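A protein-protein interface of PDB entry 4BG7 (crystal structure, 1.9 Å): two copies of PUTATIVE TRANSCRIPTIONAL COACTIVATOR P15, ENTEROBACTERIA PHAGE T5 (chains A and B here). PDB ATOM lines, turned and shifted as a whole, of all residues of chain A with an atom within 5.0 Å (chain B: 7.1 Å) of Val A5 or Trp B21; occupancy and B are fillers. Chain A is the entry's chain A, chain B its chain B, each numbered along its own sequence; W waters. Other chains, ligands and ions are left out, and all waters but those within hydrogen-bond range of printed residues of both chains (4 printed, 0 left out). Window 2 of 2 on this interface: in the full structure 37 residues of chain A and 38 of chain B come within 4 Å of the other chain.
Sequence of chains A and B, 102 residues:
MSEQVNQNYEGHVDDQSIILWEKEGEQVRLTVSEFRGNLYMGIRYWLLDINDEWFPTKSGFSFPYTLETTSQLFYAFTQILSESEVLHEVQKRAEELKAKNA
Hydrophobic or aromatic side chains of chain A within 4 Å of the printed part of chain B: Val A5, Phe A63 and Pro A64.
Printed residues of chain B that touch a printed residue of chain A: Trp B21, Lys B23, Val B28, Tyr B45 and Ser B59.
CA of Gln A4 touches CZ2 of Trp B21, at 3.9 Å.
Val A5 touches Trp B21.
Val A5 touches Val B28 (CG2 to CG2, 3.5 Å).
Val A5 touches Tyr B45 (CB to CE1, 3.6 Å).
OE1 of Gln A7 touches CE2 of Tyr B45, 3.8 Å away.
Ser B59 touches Gln A7 (OG to CG, 3.3 Å).
Trp B21 touches Phe A63 (CB to CD2, 3.97 Å).
Trp B21 touches Pro A64 (NE1 to CG, 3.5 Å).
Trp B21 touches Thr A69.
The indole nitrogen (NE1) of Trp B21 sits at hydrogen-bond distance from the side-chain carboxylate (OE1) of Glu A3, 3.0 Å away.
NZ of Lys B23 sits at hydrogen-bond distance from O of Glu A3.
The backbone NH (N) of Leu B20 sits at hydrogen-bond distance from the backbone carbonyl oxygen (O) of Val B28.
N of Val B28 sits at hydrogen-bond distance from O of Trp B21, 2.9 Å away.
The side-chain hydroxyl (OH) of Tyr B45 is in hydrogen-bond range of the side-chain carboxylate (OE1) of Glu B26, 2.5 Å away.
OG1 of Thr B57 is in hydrogen-bond range of O of Tyr B45, 2.7 Å away.
N of Tyr B45 sits at hydrogen-bond distance from O of Ser B59 (2.8 Å).
The side-chain hydroxyl (OG1) of Thr B57 lies close to the backbone NH (N) of Ser B59 (3.1 Å).
Val A5 touches three residues of chain B.
Of chain A, only Glu A3, Gln A4, Val A5, Phe A63, Pro A64 and Thr A69 come within 4 Å of Trp B21.
Of the printed residues of chain B, Phe A63 touches Trp B21.
Printed residues of chain A within 4 Å of Tyr B45: Val A5 (3.6 Å) and Gln A7 (3.8 Å).
Gln B27 touches none of the printed residues of chain A.
The nearest printed residue of chain A that does not touch Trp B21 is Ser A62 (7.3 Å).
The nearest printed residue of chain B that does not touch Phe A63 is Val B28 (4.1 Å).
No position is printed for both chains.
Of the 11 pairs that touch across the chains among the printed residues, none has its exchanged pair printed and touching as well.
Water W4 bridges NE2 of Gln A7 (2.5 Å) and OG of Ser B59 (2.7 Å).
Water W2 lies within hydrogen-bond range of OE1 of Glu B26 and N of Val A5.
Water W3 bridges the side-chain carboxylate (OE1) of Glu A3 (2.8 Å) and the indole nitrogen (NE1) of Trp B21 (3.3 Å).
Water W1 lies within hydrogen-bond range of OG of Ser B59 and O of Gln A7.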
ATOM      1  N   GLU A   3      26.287  -8.421 -19.450  1.00  0.00           N
ATOM      2  CA  GLU A   3      26.268  -9.651 -20.359  1.00  0.00           C
ATOM      3  C   GLU A   3      26.623 -10.926 -19.581  1.00  0.00           C
ATOM      4  O   GLU A   3      27.816 -11.236 -19.395  1.00  0.00           O
ATOM      5  CB  GLU A   3      27.278  -9.540 -21.540  1.00  0.00           C
ATOM      6  CG  GLU A   3      26.909  -8.736 -22.777  1.00  0.00           C
ATOM      7  CD  GLU A   3      25.896  -9.434 -23.707  1.00  0.00           C
ATOM      8  OE1 GLU A   3      25.873 -10.683 -23.845  1.00  0.00           O
ATOM      9  OE2 GLU A   3      25.103  -8.698 -24.296  1.00  0.00           O
ATOM     10  N   GLN A   4      25.612 -11.675 -19.144  1.00  0.00           N
ATOM     11  CA  GLN A   4      25.815 -12.791 -18.193  1.00  0.00           C
ATOM     12  C   GLN A   4      24.606 -13.750 -18.136  1.00  0.00           C
ATOM     13  O   GLN A   4      23.541 -13.332 -18.508  1.00  0.00           O
ATOM     14  CB  GLN A   4      26.002 -12.194 -16.802  1.00  0.00           C
ATOM     15  CG  GLN A   4      24.692 -11.819 -16.148  1.00  0.00           C
ATOM     16  CD  GLN A   4      24.804 -10.779 -15.066  1.00  0.00           C
ATOM     17  OE1 GLN A   4      25.436  -9.741 -15.253  1.00  0.00           O
ATOM     18  NE2 GLN A   4      24.143 -11.031 -13.936  1.00  0.00           N
ATOM     19  N   VAL A   5      24.777 -14.973 -17.612  1.00  0.00           N
ATOM     20  CA  VAL A   5      23.652 -15.901 -17.323  1.00  0.00           C
ATOM     21  C   VAL A   5      23.276 -15.864 -15.820  1.00  0.00           C
ATOM     22  O   VAL A   5      24.141 -15.790 -14.927  1.00  0.00           O
ATOM     23  CB  VAL A   5      23.935 -17.365 -17.777  1.00  0.00           C
ATOM     24  CG1 VAL A   5      22.882 -18.365 -17.231  1.00  0.00           C
ATOM     25  CG2 VAL A   5      24.020 -17.459 -19.305  1.00  0.00           C
ATOM     26  N   ASN A   6      21.975 -15.835 -15.558  1.00  0.00           N
ATOM     27  CA  ASN A   6      21.472 -15.848 -14.193  1.00  0.00           C
ATOM     28  C   ASN A   6      20.874 -17.186 -13.875  1.00  0.00           C
ATOM     29  O   ASN A   6      20.124 -17.723 -14.708  1.00  0.00           O
ATOM     30  CB  ASN A   6      20.444 -14.744 -13.997  1.00  0.00           C
ATOM     31  CG  ASN A   6      20.924 -13.428 -14.508  1.00  0.00           C
ATOM     32  OD1 ASN A   6      21.830 -12.872 -13.958  1.00  0.00           O
ATOM     33  ND2 ASN A   6      20.342 -12.951 -15.609  1.00  0.00           N
ATOM     34  N   GLN A   7      21.193 -17.700 -12.658  1.00  0.00           N
ATOM     35  CA  GLN A   7      20.827 -19.069 -12.243  1.00  0.00           C
ATOM     36  C   GLN A   7      19.592 -19.058 -11.363  1.00  0.00           C
ATOM     37  O   GLN A   7      19.095 -20.114 -10.927  1.00  0.00           O
ATOM     38  CB  GLN A   7      22.048 -19.823 -11.672  1.00  0.00           C
ATOM     39  CG  GLN A   7      23.141 -20.030 -12.745  1.00  0.00           C
ATOM     40  CD  GLN A   7      24.432 -20.667 -12.179  1.00  0.00           C
ATOM     41  OE1 GLN A   7      25.473 -20.026 -12.083  1.00  0.00           O
ATOM     42  NE2 GLN A   7      24.337 -21.906 -11.763  1.00  0.00           N
ATOM     43  N   SER A  62      18.112 -17.232 -16.868  1.00  0.00           N
ATOM     44  CA  SER A  62      17.956 -16.295 -17.907  1.00  0.00           C
ATOM     45  C   SER A  62      19.292 -15.957 -18.511  1.00  0.00           C
ATOM     46  O   SER A  62      20.382 -16.297 -17.950  1.00  0.00           O
ATOM     47  CB  SER A  62      17.221 -15.068 -17.370  1.00  0.00           C
ATOM     48  OG  SER A  62      17.953 -14.359 -16.394  1.00  0.00           O
ATOM     49  N   PHE A  63      19.234 -15.337 -19.677  1.00  0.00           N
ATOM     50  CA  PHE A  63      20.449 -14.884 -20.306  1.00  0.00           C
ATOM     51  C   PHE A  63      20.157 -13.608 -21.095  1.00  0.00           C
ATOM     52  O   PHE A  63      19.015 -13.221 -21.242  1.00  0.00           O
ATOM     53  CB  PHE A  63      21.102 -16.010 -21.126  1.00  0.00           C
ATOM     54  CG  PHE A  63      20.345 -16.396 -22.350  1.00  0.00           C
ATOM     55  CD1 PHE A  63      19.220 -17.179 -22.247  1.00  0.00           C
ATOM     56  CD2 PHE A  63      20.796 -16.052 -23.604  1.00  0.00           C
ATOM     57  CE1 PHE A  63      18.495 -17.606 -23.356  1.00  0.00           C
ATOM     58  CE2 PHE A  63      20.089 -16.460 -24.733  1.00  0.00           C
ATOM     59  CZ  PHE A  63      18.915 -17.224 -24.602  1.00  0.00           C
ATOM     60  N   PRO A  64      21.182 -12.932 -21.618  1.00  0.00           N
ATOM     61  CA  PRO A  64      20.826 -11.617 -22.143  1.00  0.00           C
ATOM     62  C   PRO A  64      19.823 -11.553 -23.301  1.00  0.00           C
ATOM     63  O   PRO A  64      19.763 -12.413 -24.186  1.00  0.00           O
ATOM     64  CB  PRO A  64      22.178 -11.017 -22.595  1.00  0.00           C
ATOM     65  CG  PRO A  64      23.208 -11.828 -21.938  1.00  0.00           C
ATOM     66  CD  PRO A  64      22.619 -13.154 -21.573  1.00  0.00           C
ATOM     67  N   THR A  69      21.338 -11.921 -29.276  1.00  0.00           N
ATOM     68  CA  THR A  69      20.870 -13.194 -28.739  1.00  0.00           C
ATOM     69  C   THR A  69      19.506 -13.568 -29.319  1.00  0.00           C
ATOM     70  O   THR A  69      19.239 -14.760 -29.595  1.00  0.00           O
ATOM     71  CB  THR A  69      20.841 -13.233 -27.194  1.00  0.00           C
ATOM     72  OG1 THR A  69      19.937 -12.226 -26.741  1.00  0.00           O
ATOM     73  CG2 THR A  69      22.229 -12.987 -26.611  1.00  0.00           C
ATOM     74  N   ILE B  18      23.240 -25.942 -31.020  1.00  0.00           N
ATOM     75  CA  ILE B  18      23.653 -24.637 -31.544  1.00  0.00           C
ATOM     76  C   ILE B  18      23.871 -23.670 -30.373  1.00  0.00           C
ATOM     77  O   ILE B  18      23.038 -23.599 -29.496  1.00  0.00           O
ATOM     78  CB  ILE B  18      22.550 -24.085 -32.463  1.00  0.00           C
ATOM     79  CG1 ILE B  18      22.274 -25.117 -33.606  1.00  0.00           C
ATOM     80  CG2 ILE B  18      22.968 -22.686 -33.009  1.00  0.00           C
ATOM     81  CD1 ILE B  18      21.111 -24.718 -34.512  1.00  0.00           C
ATOM     82  N   ILE B  19      24.990 -22.972 -30.355  1.00  0.00           N
ATOM     83  CA  ILE B  19      25.290 -21.991 -29.318  1.00  0.00           C
ATOM     84  C   ILE B  19      24.438 -20.730 -29.497  1.00  0.00           C
ATOM     85  O   ILE B  19      24.398 -20.128 -30.580  1.00  0.00           O
ATOM     86  CB  ILE B  19      26.795 -21.676 -29.283  1.00  0.00           C
ATOM     87  CG1 ILE B  19      27.567 -22.960 -28.916  1.00  0.00           C
ATOM     88  CG2 ILE B  19      27.080 -20.584 -28.253  1.00  0.00           C
ATOM     89  CD1 ILE B  19      28.985 -23.142 -29.481  1.00  0.00           C
ATOM     90  N   LEU B  20      23.728 -20.344 -28.450  1.00  0.00           N
ATOM     91  CA  LEU B  20      22.866 -19.103 -28.452  1.00  0.00           C
ATOM     92  C   LEU B  20      23.612 -17.900 -27.908  1.00  0.00           C
ATOM     93  O   LEU B  20      23.295 -16.731 -28.220  1.00  0.00           O
ATOM     94  CB  LEU B  20      21.612 -19.295 -27.615  1.00  0.00           C
ATOM     95  CG  LEU B  20      20.651 -20.388 -28.062  1.00  0.00           C
ATOM     96  CD1 LEU B  20      19.380 -20.374 -27.239  1.00  0.00           C
ATOM     97  CD2 LEU B  20      20.357 -20.162 -29.558  1.00  0.00           C
ATOM     98  N   TRP B  21      24.558 -18.186 -27.045  1.00  0.00           N
ATOM     99  CA  TRP B  21      25.271 -17.159 -26.332  1.00  0.00           C
ATOM    100  C   TRP B  21      26.447 -17.795 -25.656  1.00  0.00           C
ATOM    101  O   TRP B  21      26.362 -18.946 -25.237  1.00  0.00           O
ATOM    102  CB  TRP B  21      24.337 -16.561 -25.317  1.00  0.00           C
ATOM    103  CG  TRP B  21      25.007 -15.608 -24.384  1.00  0.00           C
ATOM    104  CD1 TRP B  21      25.079 -14.225 -24.514  1.00  0.00           C
ATOM    105  CD2 TRP B  21      25.759 -15.915 -23.199  1.00  0.00           C
ATOM    106  NE1 TRP B  21      25.772 -13.683 -23.476  1.00  0.00           N
ATOM    107  CE2 TRP B  21      26.202 -14.638 -22.656  1.00  0.00           C
ATOM    108  CE3 TRP B  21      26.095 -17.079 -22.533  1.00  0.00           C
ATOM    109  CZ2 TRP B  21      26.932 -14.554 -21.500  1.00  0.00           C
ATOM    110  CZ3 TRP B  21      26.821 -16.978 -21.361  1.00  0.00           C
ATOM    111  CH2 TRP B  21      27.243 -15.744 -20.863  1.00  0.00           C
ATOM    112  N   GLU B  22      27.572 -17.073 -25.552  1.00  0.00           N
ATOM    113  CA  GLU B  22      28.738 -17.591 -24.847  1.00  0.00           C
ATOM    114  C   GLU B  22      29.754 -16.557 -24.475  1.00  0.00           C
ATOM    115  O   GLU B  22      29.882 -15.506 -25.123  1.00  0.00           O
ATOM    116  CB  GLU B  22      29.475 -18.664 -25.665  1.00  0.00           C
ATOM    117  CG  GLU B  22      29.990 -18.194 -27.015  1.00  0.00           C
ATOM    118  CD  GLU B  22      30.757 -19.277 -27.771  1.00  0.00           C
ATOM    119  OE1 GLU B  22      31.433 -20.133 -27.148  1.00  0.00           O
ATOM    120  OE2 GLU B  22      30.668 -19.249 -29.004  1.00  0.00           O
ATOM    121  N   LYS B  23      30.495 -16.914 -23.464  1.00  0.00           N
ATOM    122  CA  LYS B  23      31.654 -16.183 -22.972  1.00  0.00           C
ATOM    123  C   LYS B  23      32.612 -17.279 -22.668  1.00  0.00           C
ATOM    124  O   LYS B  23      32.255 -18.451 -22.795  1.00  0.00           O
ATOM    125  CB  LYS B  23      31.341 -15.419 -21.655  1.00  0.00           C
ATOM    126  CG  LYS B  23      30.586 -14.126 -21.831  1.00  0.00           C
ATOM    127  CD  LYS B  23      30.705 -13.177 -20.620  1.00  0.00           C
ATOM    128  CE  LYS B  23      30.272 -13.825 -19.314  1.00  0.00           C
ATOM    129  NZ  LYS B  23      29.995 -12.799 -18.275  1.00  0.00           N
ATOM    130  N   GLU B  24      33.814 -16.921 -22.208  1.00  0.00           N
ATOM    131  CA  GLU B  24      34.820 -17.938 -21.822  1.00  0.00           C
ATOM    132  C   GLU B  24      34.317 -18.855 -20.699  1.00  0.00           C
ATOM    133  O   GLU B  24      33.923 -18.382 -19.654  1.00  0.00           O
ATOM    134  CB  GLU B  24      36.164 -17.284 -21.388  1.00  0.00           C
ATOM    135  CG  GLU B  24      37.247 -18.359 -21.277  1.00  0.00           C
ATOM    136  CD  GLU B  24      38.640 -17.856 -20.922  1.00  0.00           C
ATOM    137  OE1 GLU B  24      38.771 -16.653 -20.600  1.00  0.00           O
ATOM    138  OE2 GLU B  24      39.589 -18.691 -20.960  1.00  0.00           O
ATOM    139  N   GLU B  26      31.483 -20.492 -20.465  1.00  0.00           N
ATOM    140  CA  GLU B  26      30.030 -20.544 -20.328  1.00  0.00           C
ATOM    141  C   GLU B  26      29.336 -20.529 -21.692  1.00  0.00           C
ATOM    142  O   GLU B  26      29.692 -19.717 -22.546  1.00  0.00           O
ATOM    143  CB  GLU B  26      29.551 -19.322 -19.548  1.00  0.00           C
ATOM    144  CG  GLU B  26      30.379 -18.990 -18.334  1.00  0.00           C
ATOM    145  CD  GLU B  26      29.893 -17.749 -17.623  1.00  0.00           C
ATOM    146  OE1 GLU B  26      28.666 -17.558 -17.460  1.00  0.00           O
ATOM    147  OE2 GLU B  26      30.777 -16.965 -17.223  1.00  0.00           O
ATOM    148  N   GLN B  27      28.343 -21.383 -21.891  1.00  0.00           N
ATOM    149  CA  GLN B  27      27.544 -21.318 -23.053  1.00  0.00           C
ATOM    150  C   GLN B  27      26.073 -21.596 -22.760  1.00  0.00           C
ATOM    151  O   GLN B  27      25.751 -22.364 -21.878  1.00  0.00           O
ATOM    152  CB  GLN B  27      27.981 -22.377 -24.059  1.00  0.00           C
ATOM    153  CG  GLN B  27      29.375 -22.295 -24.637  1.00  0.00           C
ATOM    154  CD  GLN B  27      29.808 -23.607 -25.323  1.00  0.00           C
ATOM    155  OE1 GLN B  27      29.102 -24.615 -25.276  1.00  0.00           O
ATOM    156  NE2 GLN B  27      30.943 -23.576 -25.983  1.00  0.00           N
ATOM    157  N   VAL B  28      25.187 -21.005 -23.545  1.00  0.00           N
ATOM    158  CA  VAL B  28      23.776 -21.368 -23.538  1.00  0.00           C
ATOM    159  C   VAL B  28      23.543 -22.055 -24.879  1.00  0.00           C
ATOM    160  O   VAL B  28      23.855 -21.469 -25.926  1.00  0.00           O
ATOM    161  CB  VAL B  28      22.806 -20.187 -23.355  1.00  0.00           C
ATOM    162  CG1 VAL B  28      21.390 -20.689 -23.620  1.00  0.00           C
ATOM    163  CG2 VAL B  28      23.020 -19.506 -21.967  1.00  0.00           C
ATOM    164  N   ARG B  29      23.074 -23.296 -24.846  1.00  0.00           N
ATOM    165  CA  ARG B  29      22.909 -24.107 -26.040  1.00  0.00           C
ATOM    166  C   ARG B  29      21.437 -24.457 -26.290  1.00  0.00           C
ATOM    167  O   ARG B  29      20.667 -24.717 -25.360  1.00  0.00           O
ATOM    168  CB  ARG B  29      23.702 -25.409 -25.950  1.00  0.00           C
ATOM    169  CG  ARG B  29      25.137 -25.235 -25.615  1.00  0.00           C
ATOM    170  CD  ARG B  29      25.874 -26.550 -25.683  1.00  0.00           C
ATOM    171  NE  ARG B  29      27.257 -26.446 -25.180  1.00  0.00           N
ATOM    172  CZ  ARG B  29      28.040 -27.496 -24.977  1.00  0.00           C
ATOM    173  NH1 ARG B  29      27.575 -28.691 -25.232  1.00  0.00           N
ATOM    174  NH2 ARG B  29      29.284 -27.358 -24.536  1.00  0.00           N
ATOM    175  N   TYR B  45      22.099 -23.787 -19.899  1.00  0.00           N
ATOM    176  CA  TYR B  45      23.435 -23.302 -19.538  1.00  0.00           C
ATOM    177  C   TYR B  45      24.423 -24.449 -19.322  1.00  0.00           C
ATOM    178  O   TYR B  45      24.202 -25.379 -18.491  1.00  0.00           O
ATOM    179  CB  TYR B  45      23.268 -22.521 -18.290  1.00  0.00           C
ATOM    180  CG  TYR B  45      24.399 -21.710 -17.769  1.00  0.00           C
ATOM    181  CD1 TYR B  45      25.213 -20.957 -18.608  1.00  0.00           C
ATOM    182  CD2 TYR B  45      24.595 -21.618 -16.377  1.00  0.00           C
ATOM    183  CE1 TYR B  45      26.234 -20.172 -18.089  1.00  0.00           C
ATOM    184  CE2 TYR B  45      25.596 -20.813 -15.845  1.00  0.00           C
ATOM    185  CZ  TYR B  45      26.420 -20.100 -16.704  1.00  0.00           C
ATOM    186  OH  TYR B  45      27.400 -19.296 -16.168  1.00  0.00           O
ATOM    187  N   TRP B  46      25.527 -24.352 -20.035  1.00  0.00           N
ATOM    188  CA  TRP B  46      26.638 -25.279 -19.895  1.00  0.00           C
ATOM    189  C   TRP B  46      27.840 -24.603 -19.368  1.00  0.00           C
ATOM    190  O   TRP B  46      28.142 -23.463 -19.730  1.00  0.00           O
ATOM    191  CB  TRP B  46      26.992 -25.919 -21.203  1.00  0.00           C
ATOM    192  CG  TRP B  46      26.052 -26.906 -21.754  1.00  0.00           C
ATOM    193  CD1 TRP B  46      24.748 -26.717 -22.198  1.00  0.00           C
ATOM    194  CD2 TRP B  46      26.328 -28.311 -21.978  1.00  0.00           C
ATOM    195  NE1 TRP B  46      24.205 -27.869 -22.640  1.00  0.00           N
ATOM    196  CE2 TRP B  46      25.101 -28.883 -22.545  1.00  0.00           C
ATOM    197  CE3 TRP B  46      27.419 -29.123 -21.772  1.00  0.00           C
ATOM    198  CZ2 TRP B  46      25.012 -30.222 -22.923  1.00  0.00           C
ATOM    199  CZ3 TRP B  46      27.304 -30.470 -22.145  1.00  0.00           C
ATOM    200  CH2 TRP B  46      26.147 -31.004 -22.687  1.00  0.00           C
ATOM    201  N   THR B  57      24.275 -27.731 -16.852  1.00  0.00           N
ATOM    202  CA  THR B  57      23.767 -27.380 -15.550  1.00  0.00           C
ATOM    203  C   THR B  57      22.228 -27.571 -15.506  1.00  0.00           C
ATOM    204  O   THR B  57      21.550 -27.845 -16.497  1.00  0.00           O
ATOM    205  CB  THR B  57      24.142 -25.961 -15.200  1.00  0.00           C
ATOM    206  OG1 THR B  57      23.308 -25.109 -15.985  1.00  0.00           O
ATOM    207  CG2 THR B  57      25.669 -25.642 -15.363  1.00  0.00           C
ATOM    208  N   SER B  59      20.388 -25.169 -14.994  1.00  0.00           N
ATOM    209  CA  SER B  59      19.881 -23.856 -15.411  1.00  0.00           C
ATOM    210  C   SER B  59      19.534 -23.987 -16.890  1.00  0.00           C
ATOM    211  O   SER B  59      20.339 -23.671 -17.777  1.00  0.00           O
ATOM    212  CB  SER B  59      20.932 -22.762 -15.184  1.00  0.00           C
ATOM    213  OG  SER B  59      21.072 -22.412 -13.804  1.00  0.00           O
HETATM  214  O   HOH W   1      18.278 -22.386 -12.765  1.00  0.00           O
HETATM  215  O   HOH W   2      27.513 -15.273 -16.468  1.00  0.00           O
HETATM  216  O   HOH W   3      28.384 -11.811 -23.982  1.00  0.00           O
HETATM  217  O   HOH W   4      22.861 -23.840 -12.451  1.00  0.00           O
